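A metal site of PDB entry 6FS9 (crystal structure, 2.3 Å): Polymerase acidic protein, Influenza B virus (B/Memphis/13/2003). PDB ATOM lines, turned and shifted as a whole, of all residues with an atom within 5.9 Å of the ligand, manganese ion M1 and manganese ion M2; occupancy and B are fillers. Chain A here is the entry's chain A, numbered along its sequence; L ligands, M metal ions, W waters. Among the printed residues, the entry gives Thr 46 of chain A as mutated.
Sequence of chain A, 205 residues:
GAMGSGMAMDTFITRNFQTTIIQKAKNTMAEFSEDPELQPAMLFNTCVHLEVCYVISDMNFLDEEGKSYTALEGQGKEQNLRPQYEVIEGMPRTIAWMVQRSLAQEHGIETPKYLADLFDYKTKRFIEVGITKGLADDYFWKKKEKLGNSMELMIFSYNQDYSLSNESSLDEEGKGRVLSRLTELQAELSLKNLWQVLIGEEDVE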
ATOM      1  N   ALA A  25      26.490  11.941  20.493  1.00  0.00           N
ATOM      2  CA  ALA A  25      26.292  12.199  21.907  1.00  0.00           C
ATOM      3  C   ALA A  25      26.508  10.885  22.723  1.00  0.00           C
ATOM      4  O   ALA A  25      27.076  10.911  23.802  1.00  0.00           O
ATOM      5  CB  ALA A  25      24.953  12.810  22.140  1.00  0.00           C
ATOM      6  N   THR A  28      30.102  10.130  23.001  1.00  0.00           N
ATOM      7  CA  THR A  28      30.662  10.913  24.071  1.00  0.00           C
ATOM      8  C   THR A  28      30.301  10.350  25.459  1.00  0.00           C
ATOM      9  O   THR A  28      31.145  10.291  26.350  1.00  0.00           O
ATOM     10  CB  THR A  28      30.156  12.343  23.983  1.00  0.00           C
ATOM     11  OG1 THR A  28      30.587  12.875  22.738  1.00  0.00           O
ATOM     12  CG2 THR A  28      30.780  13.183  25.061  1.00  0.00           C
ATOM     13  N   MET A  29      29.054   9.955  25.663  1.00  0.00           N
ATOM     14  CA  MET A  29      28.672   9.425  26.975  1.00  0.00           C
ATOM     15  C   MET A  29      29.509   8.161  27.293  1.00  0.00           C
ATOM     16  O   MET A  29      29.921   7.953  28.416  1.00  0.00           O
ATOM     17  CB  MET A  29      27.159   9.138  27.056  1.00  0.00           C
ATOM     18  CG  MET A  29      26.285  10.369  27.222  1.00  0.00           C
ATOM     19  SD  MET A  29      24.518  10.024  26.972  1.00  0.00           S
ATOM     20  CE  MET A  29      24.066   9.163  28.489  1.00  0.00           C
ATOM     21  N   ALA A  30      29.719   7.318  26.294  1.00  0.00           N
ATOM     22  CA  ALA A  30      30.565   6.111  26.397  1.00  0.00           C
ATOM     23  C   ALA A  30      32.016   6.411  26.852  1.00  0.00           C
ATOM     24  O   ALA A  30      32.584   5.709  27.668  1.00  0.00           O
ATOM     25  CB  ALA A  30      30.561   5.334  25.059  1.00  0.00           C
ATOM     26  N   PHE A  32      32.991   8.702  28.727  1.00  0.00           N
ATOM     27  CA  PHE A  32      32.802   8.897  30.185  1.00  0.00           C
ATOM     28  C   PHE A  32      32.201   7.686  30.942  1.00  0.00           C
ATOM     29  O   PHE A  32      31.760   7.809  32.072  1.00  0.00           O
ATOM     30  CB  PHE A  32      31.954  10.190  30.395  1.00  0.00           C
ATOM     31  CG  PHE A  32      32.701  11.456  30.065  1.00  0.00           C
ATOM     32  CD1 PHE A  32      33.713  11.906  30.905  1.00  0.00           C
ATOM     33  CD2 PHE A  32      32.459  12.159  28.893  1.00  0.00           C
ATOM     34  CE1 PHE A  32      34.436  13.062  30.607  1.00  0.00           C
ATOM     35  CE2 PHE A  32      33.174  13.311  28.580  1.00  0.00           C
ATOM     36  CZ  PHE A  32      34.174  13.762  29.432  1.00  0.00           C
ATOM     37  N   GLU A  34      29.218   6.565  30.654  1.00  0.00           N
ATOM     38  CA  GLU A  34      27.807   6.709  31.000  1.00  0.00           C
ATOM     39  C   GLU A  34      27.050   5.975  29.920  1.00  0.00           C
ATOM     40  O   GLU A  34      27.420   6.005  28.754  1.00  0.00           O
ATOM     41  CB  GLU A  34      27.378   8.163  31.106  1.00  0.00           C
ATOM     42  CG  GLU A  34      28.019   8.925  32.253  1.00  0.00           C
ATOM     43  CD  GLU A  34      27.566   8.483  33.630  1.00  0.00           C
ATOM     44  OE1 GLU A  34      26.376   8.147  33.819  1.00  0.00           O
ATOM     45  OE2 GLU A  34      28.444   8.497  34.514  1.00  0.00           O
ATOM     46  N   MET A  42      20.551  12.504  30.246  1.00  0.00           N
ATOM     47  CA  MET A  42      21.851  12.963  29.813  1.00  0.00           C
ATOM     48  C   MET A  42      21.932  12.882  28.312  1.00  0.00           C
ATOM     49  O   MET A  42      22.470  13.794  27.638  1.00  0.00           O
ATOM     50  CB  MET A  42      22.943  12.125  30.456  1.00  0.00           C
ATOM     51  CG  MET A  42      24.370  12.588  30.170  1.00  0.00           C
ATOM     52  SD  MET A  42      25.573  11.625  31.078  1.00  0.00           S
ATOM     53  CE  MET A  42      25.240  12.298  32.724  1.00  0.00           C
ATOM     54  N   ASN A  45      20.102  15.877  26.876  1.00  0.00           N
ATOM     55  CA  ASN A  45      20.790  17.137  27.130  1.00  0.00           C
ATOM     56  C   ASN A  45      22.013  17.311  26.253  1.00  0.00           C
ATOM     57  O   ASN A  45      22.265  18.443  25.796  1.00  0.00           O
ATOM     58  CB  ASN A  45      21.205  17.242  28.574  1.00  0.00           C
ATOM     59  CG  ASN A  45      20.029  17.428  29.493  1.00  0.00           C
ATOM     60  OD1 ASN A  45      19.032  18.064  29.135  1.00  0.00           O
ATOM     61  ND2 ASN A  45      20.137  16.902  30.685  1.00  0.00           N
ATOM     62  N   THR A  46      22.682  16.185  25.969  1.00  0.00           N
ATOM     63  CA  THR A  46      23.896  16.203  25.180  1.00  0.00           C
ATOM     64  C   THR A  46      23.495  16.345  23.734  1.00  0.00           C
ATOM     65  O   THR A  46      24.211  16.982  22.964  1.00  0.00           O
ATOM     66  CB  THR A  46      24.817  14.974  25.396  1.00  0.00           C
ATOM     67  OG1 THR A  46      24.083  13.783  25.245  1.00  0.00           O
ATOM     68  CG2 THR A  46      25.397  14.952  26.794  1.00  0.00           C
ATOM     69  N   HIS A  49      22.642  20.096  23.269  1.00  0.00           N
ATOM     70  CA  HIS A  49      23.861  20.931  23.311  1.00  0.00           C
ATOM     71  C   HIS A  49      24.617  20.809  22.007  1.00  0.00           C
ATOM     72  O   HIS A  49      24.952  21.811  21.386  1.00  0.00           O
ATOM     73  CB  HIS A  49      24.715  20.482  24.449  1.00  0.00           C
ATOM     74  CG  HIS A  49      26.026  21.188  24.570  1.00  0.00           C
ATOM     75  ND1 HIS A  49      27.192  20.624  24.133  1.00  0.00           N
ATOM     76  CD2 HIS A  49      26.372  22.324  25.179  1.00  0.00           C
ATOM     77  CE1 HIS A  49      28.191  21.413  24.414  1.00  0.00           C
ATOM     78  NE2 HIS A  49      27.726  22.466  25.044  1.00  0.00           N
ATOM     79  N   CYS A  53      25.211  23.654  19.011  1.00  0.00           N
ATOM     80  CA  CYS A  53      26.527  23.905  18.438  1.00  0.00           C
ATOM     81  C   CYS A  53      26.473  23.856  16.935  1.00  0.00           C
ATOM     82  O   CYS A  53      26.934  24.794  16.270  1.00  0.00           O
ATOM     83  CB  CYS A  53      27.573  22.893  18.922  1.00  0.00           C
ATOM     84  SG  CYS A  53      28.036  23.034  20.662  1.00  0.00           S
ATOM     85  N   GLU A  89      33.097  20.225  19.853  1.00  0.00           N
ATOM     86  CA  GLU A  89      32.199  19.306  20.548  1.00  0.00           C
ATOM     87  C   GLU A  89      31.791  18.166  19.591  1.00  0.00           C
ATOM     88  O   GLU A  89      31.775  18.347  18.380  1.00  0.00           O
ATOM     89  CB  GLU A  89      30.942  20.051  21.049  1.00  0.00           C
ATOM     90  CG  GLU A  89      30.009  19.211  21.964  1.00  0.00           C
ATOM     91  CD  GLU A  89      30.753  18.519  23.120  1.00  0.00           C
ATOM     92  OE1 GLU A  89      30.703  19.077  24.256  1.00  0.00           O
ATOM     93  OE2 GLU A  89      31.387  17.432  22.895  1.00  0.00           O
ATOM     94  N   ARG A  93      37.620  12.996  22.699  1.00  0.00           N
ATOM     95  CA  ARG A  93      38.474  13.988  23.345  1.00  0.00           C
ATOM     96  C   ARG A  93      39.912  14.037  22.841  1.00  0.00           C
ATOM     97  O   ARG A  93      40.504  15.123  22.810  1.00  0.00           O
ATOM     98  CB  ARG A  93      38.433  13.844  24.867  1.00  0.00           C
ATOM     99  CG  ARG A  93      37.102  14.311  25.379  1.00  0.00           C
ATOM    100  CD  ARG A  93      37.087  14.346  26.879  1.00  0.00           C
ATOM    101  NE  ARG A  93      37.756  15.521  27.424  1.00  0.00           N
ATOM    102  CZ  ARG A  93      37.155  16.676  27.650  1.00  0.00           C
ATOM    103  NH1 ARG A  93      35.893  16.860  27.336  1.00  0.00           N
ATOM    104  NH2 ARG A  93      37.799  17.683  28.201  1.00  0.00           N
ATOM    105  N   LEU A 115      38.556  22.136  27.242  1.00  0.00           N
ATOM    106  CA  LEU A 115      38.107  21.836  25.880  1.00  0.00           C
ATOM    107  C   LEU A 115      36.863  22.641  25.551  1.00  0.00           C
ATOM    108  O   LEU A 115      35.942  22.657  26.332  1.00  0.00           O
ATOM    109  CB  LEU A 115      37.809  20.347  25.752  1.00  0.00           C
ATOM    110  CG  LEU A 115      37.651  19.751  24.364  1.00  0.00           C
ATOM    111  CD1 LEU A 115      39.002  19.756  23.677  1.00  0.00           C
ATOM    112  CD2 LEU A 115      37.116  18.326  24.450  1.00  0.00           C
ATOM    113  N   ALA A 116      36.879  23.335  24.423  1.00  0.00           N
ATOM    114  CA  ALA A 116      35.810  24.221  23.973  1.00  0.00           C
ATOM    115  C   ALA A 116      34.785  23.472  23.160  1.00  0.00           C
ATOM    116  O   ALA A 116      34.986  22.332  22.760  1.00  0.00           O
ATOM    117  CB  ALA A 116      36.399  25.324  23.118  1.00  0.00           C
ATOM    118  N   ASP A 117      33.720  24.174  22.864  1.00  0.00           N
ATOM    119  CA  ASP A 117      32.635  23.652  22.017  1.00  0.00           C
ATOM    120  C   ASP A 117      32.830  24.089  20.599  1.00  0.00           C
ATOM    121  O   ASP A 117      32.612  23.265  19.706  1.00  0.00           O
ATOM    122  CB  ASP A 117      31.284  24.092  22.545  1.00  0.00           C
ATOM    123  CG  ASP A 117      30.933  23.413  23.892  1.00  0.00           C
ATOM    124  OD1 ASP A 117      31.342  22.258  24.011  1.00  0.00           O
ATOM    125  OD2 ASP A 117      30.263  23.998  24.816  1.00  0.00           O
ATOM    126  N   GLU A 128      32.586  28.462  24.418  1.00  0.00           N
ATOM    127  CA  GLU A 128      31.884  27.512  25.244  1.00  0.00           C
ATOM    128  C   GLU A 128      30.381  27.842  25.054  1.00  0.00           C
ATOM    129  O   GLU A 128      29.938  28.963  25.272  1.00  0.00           O
ATOM    130  CB  GLU A 128      32.258  27.677  26.713  1.00  0.00           C
ATOM    131  CG  GLU A 128      31.386  26.833  27.691  1.00  0.00           C
ATOM    132  CD  GLU A 128      31.485  25.312  27.411  1.00  0.00           C
ATOM    133  OE1 GLU A 128      32.575  24.879  26.971  1.00  0.00           O
ATOM    134  OE2 GLU A 128      30.503  24.563  27.596  1.00  0.00           O
ATOM    135  N   VAL A 129      29.620  26.809  24.668  1.00  0.00           N
ATOM    136  CA  VAL A 129      28.185  26.824  24.573  1.00  0.00           C
ATOM    137  C   VAL A 129      27.597  26.169  25.804  1.00  0.00           C
ATOM    138  O   VAL A 129      28.061  25.109  26.260  1.00  0.00           O
ATOM    139  CB  VAL A 129      27.702  26.089  23.326  1.00  0.00           C
ATOM    140  CG1 VAL A 129      26.206  26.114  23.232  1.00  0.00           C
ATOM    141  CG2 VAL A 129      28.359  26.654  22.053  1.00  0.00           C
ATOM    142  N   GLY A 130      26.593  26.835  26.362  1.00  0.00           N
ATOM    143  CA  GLY A 130      25.879  26.378  27.546  1.00  0.00           C
ATOM    144  C   GLY A 130      24.365  26.383  27.328  1.00  0.00           C
ATOM    145  O   GLY A 130      23.808  27.317  26.718  1.00  0.00           O
ATOM    146  N   ILE A 131      23.699  25.344  27.819  1.00  0.00           N
ATOM    147  CA  ILE A 131      22.229  25.275  27.749  1.00  0.00           C
ATOM    148  C   ILE A 131      21.721  25.123  29.147  1.00  0.00           C
ATOM    149  O   ILE A 131      22.196  24.307  29.865  1.00  0.00           O
ATOM    150  CB  ILE A 131      21.732  24.090  26.923  1.00  0.00           C
ATOM    151  CG1 ILE A 131      22.393  24.019  25.547  1.00  0.00           C
ATOM    152  CG2 ILE A 131      20.218  24.171  26.720  1.00  0.00           C
ATOM    153  CD1 ILE A 131      22.055  25.140  24.612  1.00  0.00           C
ATOM    154  N   TYR A 139      23.957  30.863  34.788  1.00  0.00           N
ATOM    155  CA  TYR A 139      24.798  29.850  34.148  1.00  0.00           C
ATOM    156  C   TYR A 139      26.030  30.503  33.452  1.00  0.00           C
ATOM    157  O   TYR A 139      27.115  29.962  33.471  1.00  0.00           O
ATOM    158  CB  TYR A 139      23.940  28.977  33.208  1.00  0.00           C
ATOM    159  CG  TYR A 139      24.553  27.657  32.775  1.00  0.00           C
ATOM    160  CD1 TYR A 139      25.165  26.782  33.684  1.00  0.00           C
ATOM    161  CD2 TYR A 139      24.523  27.273  31.458  1.00  0.00           C
ATOM    162  CE1 TYR A 139      25.744  25.584  33.258  1.00  0.00           C
ATOM    163  CE2 TYR A 139      25.061  26.079  31.030  1.00  0.00           C
ATOM    164  CZ  TYR A 139      25.683  25.250  31.911  1.00  0.00           C
ATOM    165  OH  TYR A 139      26.219  24.091  31.410  1.00  0.00           O
ATOM    166  N   LYS A 143      29.934  29.409  34.573  1.00  0.00           N
ATOM    167  CA  LYS A 143      30.871  28.999  33.527  1.00  0.00           C
ATOM    168  C   LYS A 143      32.144  29.851  33.599  1.00  0.00           C
ATOM    169  O   LYS A 143      33.243  29.343  33.460  1.00  0.00           O
ATOM    170  CB  LYS A 143      30.253  29.140  32.157  1.00  0.00           C
ATOM    171  CG  LYS A 143      29.245  28.068  31.806  1.00  0.00           C
ATOM    172  CD  LYS A 143      29.899  26.878  31.113  1.00  0.00           C
ATOM    173  CE  LYS A 143      28.875  25.813  30.728  1.00  0.00           C
ATOM    174  NZ  LYS A 143      29.452  24.645  29.995  1.00  0.00           N
HETATM  175  C1  LIG L   1      28.597  21.801  28.726  1.00  0.00           C
HETATM  176  N1  LIG L   1      29.288  19.315  29.765  1.00  0.00           N
HETATM  177  O1  LIG L   1      28.321  22.899  28.218  1.00  0.00           O
HETATM  178  C2  LIG L   1      27.872  21.229  29.746  1.00  0.00           C
HETATM  179  O2  LIG L   1      30.330  21.610  27.241  1.00  0.00           O
HETATM  180  O3  LIG L   1      31.965  19.326  27.285  1.00  0.00           O
HETATM  181  C3  LIG L   1      30.051  19.812  28.686  1.00  0.00           C
HETATM  182  O4  LIG L   1      33.001  17.718  31.423  1.00  0.00           O
HETATM  183  C4  LIG L   1      29.730  21.065  28.169  1.00  0.00           C
HETATM  184  C5  LIG L   1      31.241  18.988  28.209  1.00  0.00           C
HETATM  185  C6  LIG L   1      30.885  17.541  30.187  1.00  0.00           C
HETATM  186  C7  LIG L   1      28.538  15.031  30.693  1.00  0.00           C
HETATM  187  C8  LIG L   1      28.092  15.907  31.860  1.00  0.00           C
HETATM  188  C9  LIG L   1      26.318  17.291  29.969  1.00  0.00           C
HETATM  189  C10 LIG L   1      27.348  17.508  29.055  1.00  0.00           C
HETATM  190  C11 LIG L   1      25.070  17.854  29.694  1.00  0.00           C
HETATM  191  C12 LIG L   1      24.843  18.588  28.534  1.00  0.00           C
HETATM  192  C13 LIG L   1      25.856  18.776  27.621  1.00  0.00           C
HETATM  193  C14 LIG L   1      27.101  18.241  27.891  1.00  0.00           C
HETATM  194  C15 LIG L   1      29.073  14.708  28.359  1.00  0.00           C
HETATM  195  C16 LIG L   1      29.161  13.305  28.545  1.00  0.00           C
HETATM  196  C17 LIG L   1      28.927  12.793  29.823  1.00  0.00           C
HETATM  197  C18 LIG L   1      28.628  13.639  30.863  1.00  0.00           C
HETATM  198  F1  LIG L   1      28.984  11.511  30.112  1.00  0.00           F
HETATM  199  C19 LIG L   1      28.766  15.581  29.428  1.00  0.00           C
HETATM  200  F2  LIG L   1      28.418  13.051  32.043  1.00  0.00           F
HETATM  201  S1  LIG L   1      26.402  16.444  31.439  1.00  0.00           S
HETATM  202  C20 LIG L   1      28.728  17.058  29.201  1.00  0.00           C
HETATM  203  N2  LIG L   1      29.492  17.977  30.188  1.00  0.00           N
HETATM  204  C21 LIG L   1      31.601  18.111  31.431  1.00  0.00           C
HETATM  205  C22 LIG L   1      33.663  17.982  30.129  1.00  0.00           C
HETATM  206  C23 LIG L   1      32.919  17.312  28.936  1.00  0.00           C
HETATM  207  N3  LIG L   1      31.626  17.968  28.986  1.00  0.00           N
HETATM  208  C24 LIG L   1      28.257  19.978  30.245  1.00  0.00           C
HETATM  209 MN    MN M   1      29.200  23.379  26.352  1.00  0.00          MN
HETATM  210 MN    MN M   2      31.857  20.826  25.479  1.00  0.00          MN
HETATM  211  O   HOH W   1      25.491  23.306  28.821  1.00  0.00           O
HETATM  212  O   HOH W   2      33.716  20.244  24.336  1.00  0.00           O
HETATM  213  O   HOH W   3      33.037  22.452  26.805  1.00  0.00           O
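Lys 143 touches manganese ion M1.
Along chain A the residues within 4 Å of manganese ion M1 span positions 49 to 143.
The nearest printed residue that does not touch manganese ion M1 is Gly 130 (4.3 Å).
Manganese ion M2 is bound by OD1 of Asp 117 (2.1 Å), water W2 (2.3 Å), O3 of the ligand (2.4 Å), water W3 (2.4 Å), OE1 of Glu 89 (2.4 Å) and O2 of the ligand (2.5 Å).
Manganese ion M2 has six donor atoms within binding distance.
The side-chain sulfur (SD) of Met 42 lies close to a fluorine (F2) of the ligand.
Residues that only touch the ligand: Thr 28, Met 29, Phe 32, Glu 34, Asn 45, Thr 46, Arg 93 and Tyr 139.
Hydrophobic or aromatic side chains within 4 Å of the ligand: Phe 32, Met 42 and His 49.
15 residues have an atom within 4 Å of the ligand: Thr 28, Met 29, Phe 32, Glu 34, Met 42, Asn 45, Thr 46, His 49, Glu 89, Arg 93, Asp 117, Glu 128, Val 129, Tyr 139 and Lys 143.
Within 4 Å of manganese ion M2: His 49, Glu 89 and Asp 117.
NZ of Lys 143 lies close to O1 of the ligand (2.7 Å).
The side-chain carboxylate of Glu 128 lies close to the side-chain amino group of Lys 143 (2.6 Å).
SG of Cys 53 is in hydrogen-bond range of O of His 49 (3.4 Å).
O of Met 42 sits at hydrogen-bond distance from OG1 of Thr 46, at 2.9 Å.
The backbone carbonyl oxygen (O) of Met 29 is in hydrogen-bond range of the backbone NH (N) of Glu 34.
Manganese ion M1 is bound by the side-chain carboxylate of Asp 117 (2.0 Å), the backbone carbonyl oxygen of Val 129 (2.1 Å), an oxygen (O1) of the ligand (2.1 Å), the side-chain carboxylate of Glu 128 (2.2 Å), a ring nitrogen (NE2) of His 49 (2.2 Å) and an oxygen (O2) of the ligand (2.3 Å).
Water W3 bridges the side-chain carboxylate of Glu 128 and the backbone carbonyl oxygen of Leu 115.
Water W1 bridges the side-chain hydroxyl (OH) of Tyr 139 (2.8 Å) and the backbone NH (N) of Ile 131 (2.9 Å).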
